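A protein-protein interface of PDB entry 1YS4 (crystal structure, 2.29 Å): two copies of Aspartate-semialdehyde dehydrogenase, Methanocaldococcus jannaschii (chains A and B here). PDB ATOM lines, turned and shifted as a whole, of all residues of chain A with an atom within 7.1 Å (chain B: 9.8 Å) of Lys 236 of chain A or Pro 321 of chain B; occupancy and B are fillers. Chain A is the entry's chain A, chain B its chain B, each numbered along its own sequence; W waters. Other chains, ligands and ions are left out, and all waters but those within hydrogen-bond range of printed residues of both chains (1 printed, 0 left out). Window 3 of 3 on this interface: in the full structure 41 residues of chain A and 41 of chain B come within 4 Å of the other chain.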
ATOM      1  N   LEU A 175      26.233   2.423  -0.235  1.00  0.00           N
ATOM      2  CA  LEU A 175      25.528   2.486   1.044  1.00  0.00           C
ATOM      3  C   LEU A 175      24.508   3.615   1.083  1.00  0.00           C
ATOM      4  O   LEU A 175      24.798   4.739   0.662  1.00  0.00           O
ATOM      5  CB  LEU A 175      26.521   2.652   2.200  1.00  0.00           C
ATOM      6  CG  LEU A 175      27.484   1.512   2.542  1.00  0.00           C
ATOM      7  CD1 LEU A 175      28.461   1.963   3.616  1.00  0.00           C
ATOM      8  CD2 LEU A 175      26.738   0.260   2.982  1.00  0.00           C
ATOM      9  N   GLU A 176      23.317   3.306   1.594  1.00  0.00           N
ATOM     10  CA  GLU A 176      22.283   4.311   1.843  1.00  0.00           C
ATOM     11  C   GLU A 176      22.144   4.584   3.341  1.00  0.00           C
ATOM     12  O   GLU A 176      22.262   5.730   3.783  1.00  0.00           O
ATOM     13  CB  GLU A 176      20.929   3.859   1.280  1.00  0.00           C
ATOM     14  CG  GLU A 176      20.875   3.701  -0.241  1.00  0.00           C
ATOM     15  CD  GLU A 176      20.583   5.004  -0.984  1.00  0.00           C
ATOM     16  OE1 GLU A 176      20.802   6.101  -0.418  1.00  0.00           O
ATOM     17  OE2 GLU A 176      20.136   4.924  -2.150  1.00  0.00           O
ATOM     18  N   ALA A 177      21.897   3.522   4.111  1.00  0.00           N
ATOM     19  CA  ALA A 177      21.599   3.636   5.540  1.00  0.00           C
ATOM     20  C   ALA A 177      22.103   2.435   6.340  1.00  0.00           C
ATOM     21  O   ALA A 177      22.042   1.292   5.878  1.00  0.00           O
ATOM     22  CB  ALA A 177      20.103   3.831   5.758  1.00  0.00           C
ATOM     23  N   VAL A 178      22.609   2.706   7.542  1.00  0.00           N
ATOM     24  CA  VAL A 178      23.131   1.663   8.426  1.00  0.00           C
ATOM     25  C   VAL A 178      22.639   1.865   9.860  1.00  0.00           C
ATOM     26  O   VAL A 178      22.829   2.934  10.448  1.00  0.00           O
ATOM     27  CB  VAL A 178      24.690   1.614   8.432  1.00  0.00           C
ATOM     28  CG1 VAL A 178      25.187   0.401   9.224  1.00  0.00           C
ATOM     29  CG2 VAL A 178      25.249   1.575   7.015  1.00  0.00           C
ATOM     30  N   PHE A 179      21.998   0.831  10.406  1.00  0.00           N
ATOM     31  CA  PHE A 179      21.661   0.786  11.821  1.00  0.00           C
ATOM     32  C   PHE A 179      22.622  -0.140  12.552  1.00  0.00           C
ATOM     33  O   PHE A 179      22.890  -1.253  12.094  1.00  0.00           O
ATOM     34  CB  PHE A 179      20.225   0.305  12.029  1.00  0.00           C
ATOM     35  CG  PHE A 179      19.189   1.371  11.819  1.00  0.00           C
ATOM     36  CD1 PHE A 179      18.974   2.347  12.782  1.00  0.00           C
ATOM     37  CD2 PHE A 179      18.422   1.391  10.660  1.00  0.00           C
ATOM     38  CE1 PHE A 179      18.010   3.335  12.591  1.00  0.00           C
ATOM     39  CE2 PHE A 179      17.453   2.375  10.461  1.00  0.00           C
ATOM     40  CZ  PHE A 179      17.245   3.344  11.428  1.00  0.00           C
ATOM     41  N   GLN A 215      28.871   7.559  14.394  1.00  0.00           N
ATOM     42  CA  GLN A 215      28.106   8.262  13.376  1.00  0.00           C
ATOM     43  C   GLN A 215      28.929   9.311  12.624  1.00  0.00           C
ATOM     44  O   GLN A 215      28.533   9.748  11.545  1.00  0.00           O
ATOM     45  CB  GLN A 215      26.841   8.875  13.991  1.00  0.00           C
ATOM     46  CG  GLN A 215      25.758   7.830  14.279  1.00  0.00           C
ATOM     47  CD  GLN A 215      24.717   8.260  15.315  1.00  0.00           C
ATOM     48  OE1 GLN A 215      23.951   7.428  15.806  1.00  0.00           O
ATOM     49  NE2 GLN A 215      24.678   9.551  15.641  1.00  0.00           N
ATOM     50  N   LEU A 219      32.143   8.292   8.575  1.00  0.00           N
ATOM     51  CA  LEU A 219      31.983   9.084   7.362  1.00  0.00           C
ATOM     52  C   LEU A 219      33.317   9.613   6.838  1.00  0.00           C
ATOM     53  O   LEU A 219      33.503   9.726   5.630  1.00  0.00           O
ATOM     54  CB  LEU A 219      30.961  10.212   7.578  1.00  0.00           C
ATOM     55  CG  LEU A 219      29.557   9.765   8.024  1.00  0.00           C
ATOM     56  CD1 LEU A 219      28.598  10.949   8.146  1.00  0.00           C
ATOM     57  CD2 LEU A 219      28.976   8.698   7.098  1.00  0.00           C
ATOM     58  N   ALA A 233      31.676  10.705   3.540  1.00  0.00           N
ATOM     59  CA  ALA A 233      30.688   9.818   2.926  1.00  0.00           C
ATOM     60  C   ALA A 233      29.270  10.316   3.208  1.00  0.00           C
ATOM     61  O   ALA A 233      29.031  10.997   4.209  1.00  0.00           O
ATOM     62  CB  ALA A 233      30.869   8.391   3.425  1.00  0.00           C
ATOM     63  N   ASN A 234      28.335   9.975   2.327  1.00  0.00           N
ATOM     64  CA  ASN A 234      26.999  10.569   2.368  1.00  0.00           C
ATOM     65  C   ASN A 234      25.864   9.638   2.778  1.00  0.00           C
ATOM     66  O   ASN A 234      24.690  10.015   2.697  1.00  0.00           O
ATOM     67  CB  ASN A 234      26.679  11.248   1.029  1.00  0.00           C
ATOM     68  CG  ASN A 234      27.556  12.457   0.767  1.00  0.00           C
ATOM     69  OD1 ASN A 234      28.424  12.432  -0.112  1.00  0.00           O
ATOM     70  ND2 ASN A 234      27.347  13.519   1.544  1.00  0.00           N
ATOM     71  N   PHE A 235      26.208   8.434   3.226  1.00  0.00           N
ATOM     72  CA  PHE A 235      25.203   7.504   3.730  1.00  0.00           C
ATOM     73  C   PHE A 235      24.781   7.862   5.155  1.00  0.00           C
ATOM     74  O   PHE A 235      25.514   8.534   5.886  1.00  0.00           O
ATOM     75  CB  PHE A 235      25.671   6.042   3.622  1.00  0.00           C
ATOM     76  CG  PHE A 235      26.815   5.684   4.537  1.00  0.00           C
ATOM     77  CD1 PHE A 235      26.570   5.146   5.801  1.00  0.00           C
ATOM     78  CD2 PHE A 235      28.136   5.859   4.129  1.00  0.00           C
ATOM     79  CE1 PHE A 235      27.623   4.807   6.647  1.00  0.00           C
ATOM     80  CE2 PHE A 235      29.192   5.522   4.966  1.00  0.00           C
ATOM     81  CZ  PHE A 235      28.936   4.997   6.229  1.00  0.00           C
ATOM     82  N   LYS A 236      23.586   7.418   5.528  1.00  0.00           N
ATOM     83  CA  LYS A 236      23.030   7.683   6.846  1.00  0.00           C
ATOM     84  C   LYS A 236      23.410   6.570   7.815  1.00  0.00           C
ATOM     85  O   LYS A 236      23.442   5.391   7.449  1.00  0.00           O
ATOM     86  CB  LYS A 236      21.510   7.818   6.762  1.00  0.00           C
ATOM     87  CG  LYS A 236      21.026   9.092   6.078  1.00  0.00           C
ATOM     88  CD  LYS A 236      19.616   8.901   5.528  1.00  0.00           C
ATOM     89  CE  LYS A 236      19.060  10.185   4.931  1.00  0.00           C
ATOM     90  NZ  LYS A 236      18.573  11.124   5.986  1.00  0.00           N
ATOM     91  N   ILE A 237      23.698   6.951   9.054  1.00  0.00           N
ATOM     92  CA  ILE A 237      24.120   5.993  10.067  1.00  0.00           C
ATOM     93  C   ILE A 237      23.544   6.331  11.450  1.00  0.00           C
ATOM     94  O   ILE A 237      23.605   7.476  11.900  1.00  0.00           O
ATOM     95  CB  ILE A 237      25.675   5.826  10.070  1.00  0.00           C
ATOM     96  CG1 ILE A 237      26.124   4.779  11.095  1.00  0.00           C
ATOM     97  CG2 ILE A 237      26.381   7.173  10.257  1.00  0.00           C
ATOM     98  CD1 ILE A 237      27.524   4.238  10.831  1.00  0.00           C
ATOM     99  N   SER A 238      22.957   5.324  12.095  1.00  0.00           N
ATOM    100  CA  SER A 238      22.391   5.477  13.434  1.00  0.00           C
ATOM    101  C   SER A 238      22.832   4.342  14.357  1.00  0.00           C
ATOM    102  O   SER A 238      22.619   3.163  14.055  1.00  0.00           O
ATOM    103  CB  SER A 238      20.865   5.534  13.372  1.00  0.00           C
ATOM    104  OG  SER A 238      20.323   5.759  14.660  1.00  0.00           O
ATOM    105  N   ALA A 239      23.437   4.710  15.483  1.00  0.00           N
ATOM    106  CA  ALA A 239      23.951   3.739  16.439  1.00  0.00           C
ATOM    107  C   ALA A 239      23.246   3.797  17.788  1.00  0.00           C
ATOM    108  O   ALA A 239      22.822   4.862  18.244  1.00  0.00           O
ATOM    109  CB  ALA A 239      25.455   3.915  16.626  1.00  0.00           C
ATOM    110  N   LYS A 257      21.292  -1.019   4.421  1.00  0.00           N
ATOM    111  CA  LYS A 257      20.629  -0.701   3.158  1.00  0.00           C
ATOM    112  C   LYS A 257      21.672  -0.241   2.144  1.00  0.00           C
ATOM    113  O   LYS A 257      22.335   0.779   2.343  1.00  0.00           O
ATOM    114  CB  LYS A 257      19.585   0.393   3.360  1.00  0.00           C
ATOM    115  CG  LYS A 257      18.692   0.659   2.155  1.00  0.00           C
ATOM    116  CD  LYS A 257      17.716   1.775   2.471  1.00  0.00           C
ATOM    117  CE  LYS A 257      16.739   2.011   1.334  1.00  0.00           C
ATOM    118  NZ  LYS A 257      15.742   3.056   1.713  1.00  0.00           N
ATOM    119  N   PHE A 323      15.610  -3.369   5.253  1.00  0.00           N
ATOM    120  CA  PHE A 323      16.756  -3.028   4.420  1.00  0.00           C
ATOM    121  C   PHE A 323      17.154  -4.254   3.591  1.00  0.00           C
ATOM    122  O   PHE A 323      16.305  -5.085   3.274  1.00  0.00           O
ATOM    123  CB  PHE A 323      17.922  -2.526   5.285  1.00  0.00           C
ATOM    124  CG  PHE A 323      17.722  -1.135   5.857  1.00  0.00           C
ATOM    125  CD1 PHE A 323      16.621  -0.355   5.501  1.00  0.00           C
ATOM    126  CD2 PHE A 323      18.670  -0.594   6.721  1.00  0.00           C
ATOM    127  CE1 PHE A 323      16.451   0.927   6.020  1.00  0.00           C
ATOM    128  CE2 PHE A 323      18.518   0.690   7.239  1.00  0.00           C
ATOM    129  CZ  PHE A 323      17.403   1.453   6.891  1.00  0.00           C
ATOM    130  N   ILE B 254      15.490   0.158  20.242  1.00  0.00           N
ATOM    131  CA  ILE B 254      14.389   0.271  19.281  1.00  0.00           C
ATOM    132  C   ILE B 254      14.524   1.542  18.437  1.00  0.00           C
ATOM    133  O   ILE B 254      14.754   2.624  18.969  1.00  0.00           O
ATOM    134  CB  ILE B 254      13.001   0.194  19.992  1.00  0.00           C
ATOM    135  CG1 ILE B 254      12.909  -1.077  20.852  1.00  0.00           C
ATOM    136  CG2 ILE B 254      11.854   0.225  18.979  1.00  0.00           C
ATOM    137  CD1 ILE B 254      11.648  -1.197  21.687  1.00  0.00           C
ATOM    138  N   PHE B 255      14.402   1.384  17.120  1.00  0.00           N
ATOM    139  CA  PHE B 255      14.482   2.484  16.160  1.00  0.00           C
ATOM    140  C   PHE B 255      13.172   2.516  15.375  1.00  0.00           C
ATOM    141  O   PHE B 255      12.815   1.529  14.728  1.00  0.00           O
ATOM    142  CB  PHE B 255      15.647   2.278  15.182  1.00  0.00           C
ATOM    143  CG  PHE B 255      16.949   1.873  15.835  1.00  0.00           C
ATOM    144  CD1 PHE B 255      17.946   2.816  16.067  1.00  0.00           C
ATOM    145  CD2 PHE B 255      17.188   0.544  16.191  1.00  0.00           C
ATOM    146  CE1 PHE B 255      19.159   2.447  16.651  1.00  0.00           C
ATOM    147  CE2 PHE B 255      18.388   0.166  16.783  1.00  0.00           C
ATOM    148  CZ  PHE B 255      19.380   1.118  17.010  1.00  0.00           C
ATOM    149  N   VAL B 256      12.463   3.643  15.427  1.00  0.00           N
ATOM    150  CA  VAL B 256      11.093   3.711  14.902  1.00  0.00           C
ATOM    151  C   VAL B 256      10.892   4.766  13.810  1.00  0.00           C
ATOM    152  O   VAL B 256      11.248   5.936  13.981  1.00  0.00           O
ATOM    153  CB  VAL B 256      10.055   3.959  16.033  1.00  0.00           C
ATOM    154  CG1 VAL B 256       8.633   3.976  15.473  1.00  0.00           C
ATOM    155  CG2 VAL B 256      10.181   2.913  17.129  1.00  0.00           C
ATOM    156  N   LYS B 257      10.316   4.328  12.692  1.00  0.00           N
ATOM    157  CA  LYS B 257       9.838   5.228  11.649  1.00  0.00           C
ATOM    158  C   LYS B 257       8.314   5.266  11.685  1.00  0.00           C
ATOM    159  O   LYS B 257       7.651   4.242  11.498  1.00  0.00           O
ATOM    160  CB  LYS B 257      10.328   4.777  10.273  1.00  0.00           C
ATOM    161  CG  LYS B 257      10.008   5.749   9.140  1.00  0.00           C
ATOM    162  CD  LYS B 257      10.768   5.359   7.890  1.00  0.00           C
ATOM    163  CE  LYS B 257      10.388   6.214   6.698  1.00  0.00           C
ATOM    164  NZ  LYS B 257      11.242   5.846   5.530  1.00  0.00           N
ATOM    165  N   PRO B 264      11.080  13.520  19.295  1.00  0.00           N
ATOM    166  CA  PRO B 264      11.305  12.722  20.508  1.00  0.00           C
ATOM    167  C   PRO B 264      10.395  13.114  21.675  1.00  0.00           C
ATOM    168  O   PRO B 264       9.932  12.239  22.410  1.00  0.00           O
ATOM    169  CB  PRO B 264      12.766  13.021  20.861  1.00  0.00           C
ATOM    170  CG  PRO B 264      13.390  13.416  19.585  1.00  0.00           C
ATOM    171  CD  PRO B 264      12.331  14.138  18.814  1.00  0.00           C
ATOM    172  N   ARG B 318      15.347   9.830  21.898  1.00  0.00           N
ATOM    173  CA  ARG B 318      16.116  10.837  21.169  1.00  0.00           C
ATOM    174  C   ARG B 318      15.877  10.745  19.659  1.00  0.00           C
ATOM    175  O   ARG B 318      15.327   9.757  19.174  1.00  0.00           O
ATOM    176  CB  ARG B 318      17.613  10.709  21.503  1.00  0.00           C
ATOM    177  CG  ARG B 318      18.250   9.386  21.078  1.00  0.00           C
ATOM    178  CD  ARG B 318      19.445   9.033  21.952  1.00  0.00           C
ATOM    179  NE  ARG B 318      20.194   7.889  21.433  1.00  0.00           N
ATOM    180  CZ  ARG B 318      19.875   6.612  21.636  1.00  0.00           C
ATOM    181  NH1 ARG B 318      20.634   5.660  21.117  1.00  0.00           N
ATOM    182  NH2 ARG B 318      18.801   6.276  22.344  1.00  0.00           N
ATOM    183  N   LYS B 319      16.282  11.787  18.933  1.00  0.00           N
ATOM    184  CA  LYS B 319      16.193  11.815  17.470  1.00  0.00           C
ATOM    185  C   LYS B 319      17.040  10.726  16.829  1.00  0.00           C
ATOM    186  O   LYS B 319      18.180  10.490  17.240  1.00  0.00           O
ATOM    187  CB  LYS B 319      16.633  13.178  16.920  1.00  0.00           C
ATOM    188  CG  LYS B 319      15.482  14.092  16.507  1.00  0.00           C
ATOM    189  CD  LYS B 319      15.966  15.336  15.757  1.00  0.00           C
ATOM    190  CE  LYS B 319      16.153  16.542  16.689  1.00  0.00           C
ATOM    191  NZ  LYS B 319      17.357  16.443  17.580  1.00  0.00           N
ATOM    192  N   ASP B 320      16.470  10.065  15.825  1.00  0.00           N
ATOM    193  CA  ASP B 320      17.214   9.135  14.993  1.00  0.00           C
ATOM    194  C   ASP B 320      17.632   9.821  13.690  1.00  0.00           C
ATOM    195  O   ASP B 320      16.800  10.443  13.029  1.00  0.00           O
ATOM    196  CB  ASP B 320      16.375   7.898  14.681  1.00  0.00           C
ATOM    197  CG  ASP B 320      17.211   6.753  14.146  1.00  0.00           C
ATOM    198  OD1 ASP B 320      17.787   6.006  14.963  1.00  0.00           O
ATOM    199  OD2 ASP B 320      17.289   6.595  12.909  1.00  0.00           O
ATOM    200  N   PRO B 321      18.925   9.724  13.327  1.00  0.00           N
ATOM    201  CA  PRO B 321      19.444  10.273  12.064  1.00  0.00           C
ATOM    202  C   PRO B 321      18.762   9.728  10.805  1.00  0.00           C
ATOM    203  O   PRO B 321      18.735  10.415   9.780  1.00  0.00           O
ATOM    204  CB  PRO B 321      20.917   9.849  12.080  1.00  0.00           C
ATOM    205  CG  PRO B 321      21.239   9.671  13.529  1.00  0.00           C
ATOM    206  CD  PRO B 321      19.997   9.110  14.134  1.00  0.00           C
ATOM    207  N   ILE B 322      18.224   8.512  10.883  1.00  0.00           N
ATOM    208  CA  ILE B 322      17.629   7.838   9.724  1.00  0.00           C
ATOM    209  C   ILE B 322      16.103   7.831   9.807  1.00  0.00           C
ATOM    210  O   ILE B 322      15.421   8.324   8.903  1.00  0.00           O
ATOM    211  CB  ILE B 322      18.153   6.383   9.573  1.00  0.00           C
ATOM    212  CG1 ILE B 322      19.687   6.352   9.595  1.00  0.00           C
ATOM    213  CG2 ILE B 322      17.595   5.734   8.304  1.00  0.00           C
ATOM    214  CD1 ILE B 322      20.292   4.957   9.622  1.00  0.00           C
ATOM    215  N   PHE B 323      15.578   7.257  10.887  1.00  0.00           N
ATOM    216  CA  PHE B 323      14.141   7.202  11.124  1.00  0.00           C
ATOM    217  C   PHE B 323      13.705   8.418  11.942  1.00  0.00           C
ATOM    218  O   PHE B 323      14.311   9.486  11.838  1.00  0.00           O
ATOM    219  CB  PHE B 323      13.756   5.890  11.824  1.00  0.00           C
ATOM    220  CG  PHE B 323      13.768   4.677  10.921  1.00  0.00           C
ATOM    221  CD1 PHE B 323      13.966   4.798   9.543  1.00  0.00           C
ATOM    222  CD2 PHE B 323      13.537   3.408  11.451  1.00  0.00           C
ATOM    223  CE1 PHE B 323      13.962   3.675   8.716  1.00  0.00           C
ATOM    224  CE2 PHE B 323      13.526   2.278  10.628  1.00  0.00           C
ATOM    225  CZ  PHE B 323      13.740   2.413   9.259  1.00  0.00           C
ATOM    226  N   ASP B 324      12.661   8.262  12.751  1.00  0.00           N
ATOM    227  CA  ASP B 324      12.154   9.359  13.573  1.00  0.00           C
ATOM    228  C   ASP B 324      12.765   9.380  14.967  1.00  0.00           C
ATOM    229  O   ASP B 324      13.275  10.410  15.414  1.00  0.00           O
ATOM    230  CB  ASP B 324      10.628   9.297  13.670  1.00  0.00           C
ATOM    231  CG  ASP B 324       9.948   9.701  12.381  1.00  0.00           C
ATOM    232  OD1 ASP B 324      10.260  10.794  11.856  1.00  0.00           O
ATOM    233  OD2 ASP B 324       9.101   8.929  11.892  1.00  0.00           O
ATOM    234  N   VAL B 325      12.716   8.236  15.646  1.00  0.00           N
ATOM    235  CA  VAL B 325      13.097   8.159  17.050  1.00  0.00           C
ATOM    236  C   VAL B 325      13.787   6.829  17.371  1.00  0.00           C
ATOM    237  O   VAL B 325      13.508   5.799  16.748  1.00  0.00           O
ATOM    238  CB  VAL B 325      11.855   8.401  17.976  1.00  0.00           C
ATOM    239  CG1 VAL B 325      10.840   7.263  17.861  1.00  0.00           C
ATOM    240  CG2 VAL B 325      12.265   8.622  19.429  1.00  0.00           C
ATOM    241  N   LYS B 326      14.716   6.875  18.321  1.00  0.00           N
ATOM    242  CA  LYS B 326      15.295   5.669  18.898  1.00  0.00           C
ATOM    243  C   LYS B 326      15.272   5.777  20.420  1.00  0.00           C
ATOM    244  O   LYS B 326      15.319   6.877  20.972  1.00  0.00           O
ATOM    245  CB  LYS B 326      16.710   5.400  18.367  1.00  0.00           C
ATOM    246  CG  LYS B 326      17.740   6.488  18.651  1.00  0.00           C
ATOM    247  CD  LYS B 326      19.079   6.145  18.018  1.00  0.00           C
ATOM    248  CE  LYS B 326      19.993   7.353  17.944  1.00  0.00           C
ATOM    249  NZ  LYS B 326      21.222   7.049  17.148  1.00  0.00           N
ATOM    250  N   TYR B 327      15.176   4.629  21.085  1.00  0.00           N
ATOM    251  CA  TYR B 327      15.081   4.581  22.540  1.00  0.00           C
ATOM    252  C   TYR B 327      15.421   3.196  23.073  1.00  0.00           C
ATOM    253  O   TYR B 327      15.515   2.227  22.310  1.00  0.00           O
ATOM    254  CB  TYR B 327      13.681   5.011  23.016  1.00  0.00           C
ATOM    255  CG  TYR B 327      12.536   4.224  22.414  1.00  0.00           C
ATOM    256  CD1 TYR B 327      12.041   3.083  23.046  1.00  0.00           C
ATOM    257  CD2 TYR B 327      11.935   4.626  21.218  1.00  0.00           C
ATOM    258  CE1 TYR B 327      10.984   2.360  22.505  1.00  0.00           C
ATOM    259  CE2 TYR B 327      10.873   3.902  20.663  1.00  0.00           C
ATOM    260  CZ  TYR B 327      10.407   2.772  21.314  1.00  0.00           C
ATOM    261  OH  TYR B 327       9.361   2.052  20.789  1.00  0.00           O
HETATM  262  O   HOH W   1      22.261   9.716  17.426  1.00  0.00           O
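OE1 of Gln 215 of chain A lies within hydrogen-bond range of NZ of Lys 326 of chain B, 3.1 Å away. OG of Ser 238 of chain A sits at hydrogen-bond distance from OD1 of Asp 320 of chain B (2.6 Å). The side-chain amino group of Lys 326 of chain B is in hydrogen-bond range of the side-chain hydroxyl of Ser 238 of chain A (2.9 Å). The backbone carbonyl oxygen (O) of Ala 239 of chain A sits at hydrogen-bond distance from the side-chain amino group (NZ) of Lys 326 of chain B.
The backbone NH of Lys 236 of chain A is in hydrogen-bond range of the backbone carbonyl oxygen of Glu 176 of chain A, 2.8 Å away. N of Val 178 of chain A is in hydrogen-bond range of O of Lys 236 of chain A (2.8 Å). The backbone NH of Ser 238 of chain A sits at hydrogen-bond distance from the backbone carbonyl oxygen of Val 178 of chain A (2.9 Å). N of Ala 239 of chain A is in hydrogen-bond range of OE1 of Gln 215 of chain A, at 2.8 Å. N of Lys 326 of chain B sits at hydrogen-bond distance from O of Arg 318 of chain B. N of Phe 323 of chain B lies within hydrogen-bond range of OD2 of Asp 320 of chain B.
Val 178 of chain A touches Ile 322 of chain B (O to CD1, 3.3 Å). CD1 of Phe 255 of chain B touches CD1 of Phe 179 of chain A, 3.5 Å away. Phe 179 of chain A touches Ile 322 of chain B. Phe 179 of chain A touches Phe 323 of chain B (CZ to CD2, 3.7 Å). Pro 321 of chain B touches Lys 236 of chain A. CG1 of Ile 322 of chain B touches CB of Lys 236 of chain A (3.7 Å). Pro 321 of chain B touches Ile 237 of chain A (CB to O, 3.6 Å). Pro 321 of chain B touches Ser 238 of chain A (CD to OG, 3.4 Å). Ser 238 of chain A touches Ile 322 of chain B. Ala 239 of chain A touches Arg 318 of chain B.
Of chain B, only Pro 321 (3.9 Å) and Ile 322 (3.7 Å) come within 4 Å of Lys 236 of chain A. No residue of chain B comes within 4 Å of Ala 177 of chain A. Val 178 of chain A touches just one residue of chain B: Ile 322. Of chain B, only Pro 321 (3.6 Å) and Ile 322 (3.98 Å) come within 4 Å of Ile 237 of chain A. Of the printed residues of chain B, Ser 238 of chain A touches Asp 320, Pro 321, Ile 322 and Lys 326. Printed residues of chain A within 4 Å of Phe 323 of chain B: Phe 179 (3.7 Å). Printed residues of chain B within 4 Å of Phe 179 of chain A: Phe 255, Asp 320, Ile 322 and Phe 323. Printed residues of chain B within 4 Å of Ala 239 of chain A: Arg 318 and Lys 326. Asn 234 of chain A touches none of the printed residues of chain B. Lys 257 of chain B touches none of the printed residues of chain A. The nearest residue of chain B that does not touch Lys 236 of chain A is Phe 323 of chain B (6.9 Å).
Among the printed residues, 16 pairs touch across the chains. Among the printed residues, no Asp or Glu carboxylate lies within 4 Å of a Lys or Arg side-chain nitrogen of the other chain.
Positions printed for both chains: 257 and 323. Of the 16 pairs that touch across the chains among the printed residues, none has its exchanged pair printed and touching as well.
Water W1 lies within hydrogen-bond range of NZ of Lys 326 of chain B (2.9 Å) and NE2 of Gln 215 of chain A (3.0 Å).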
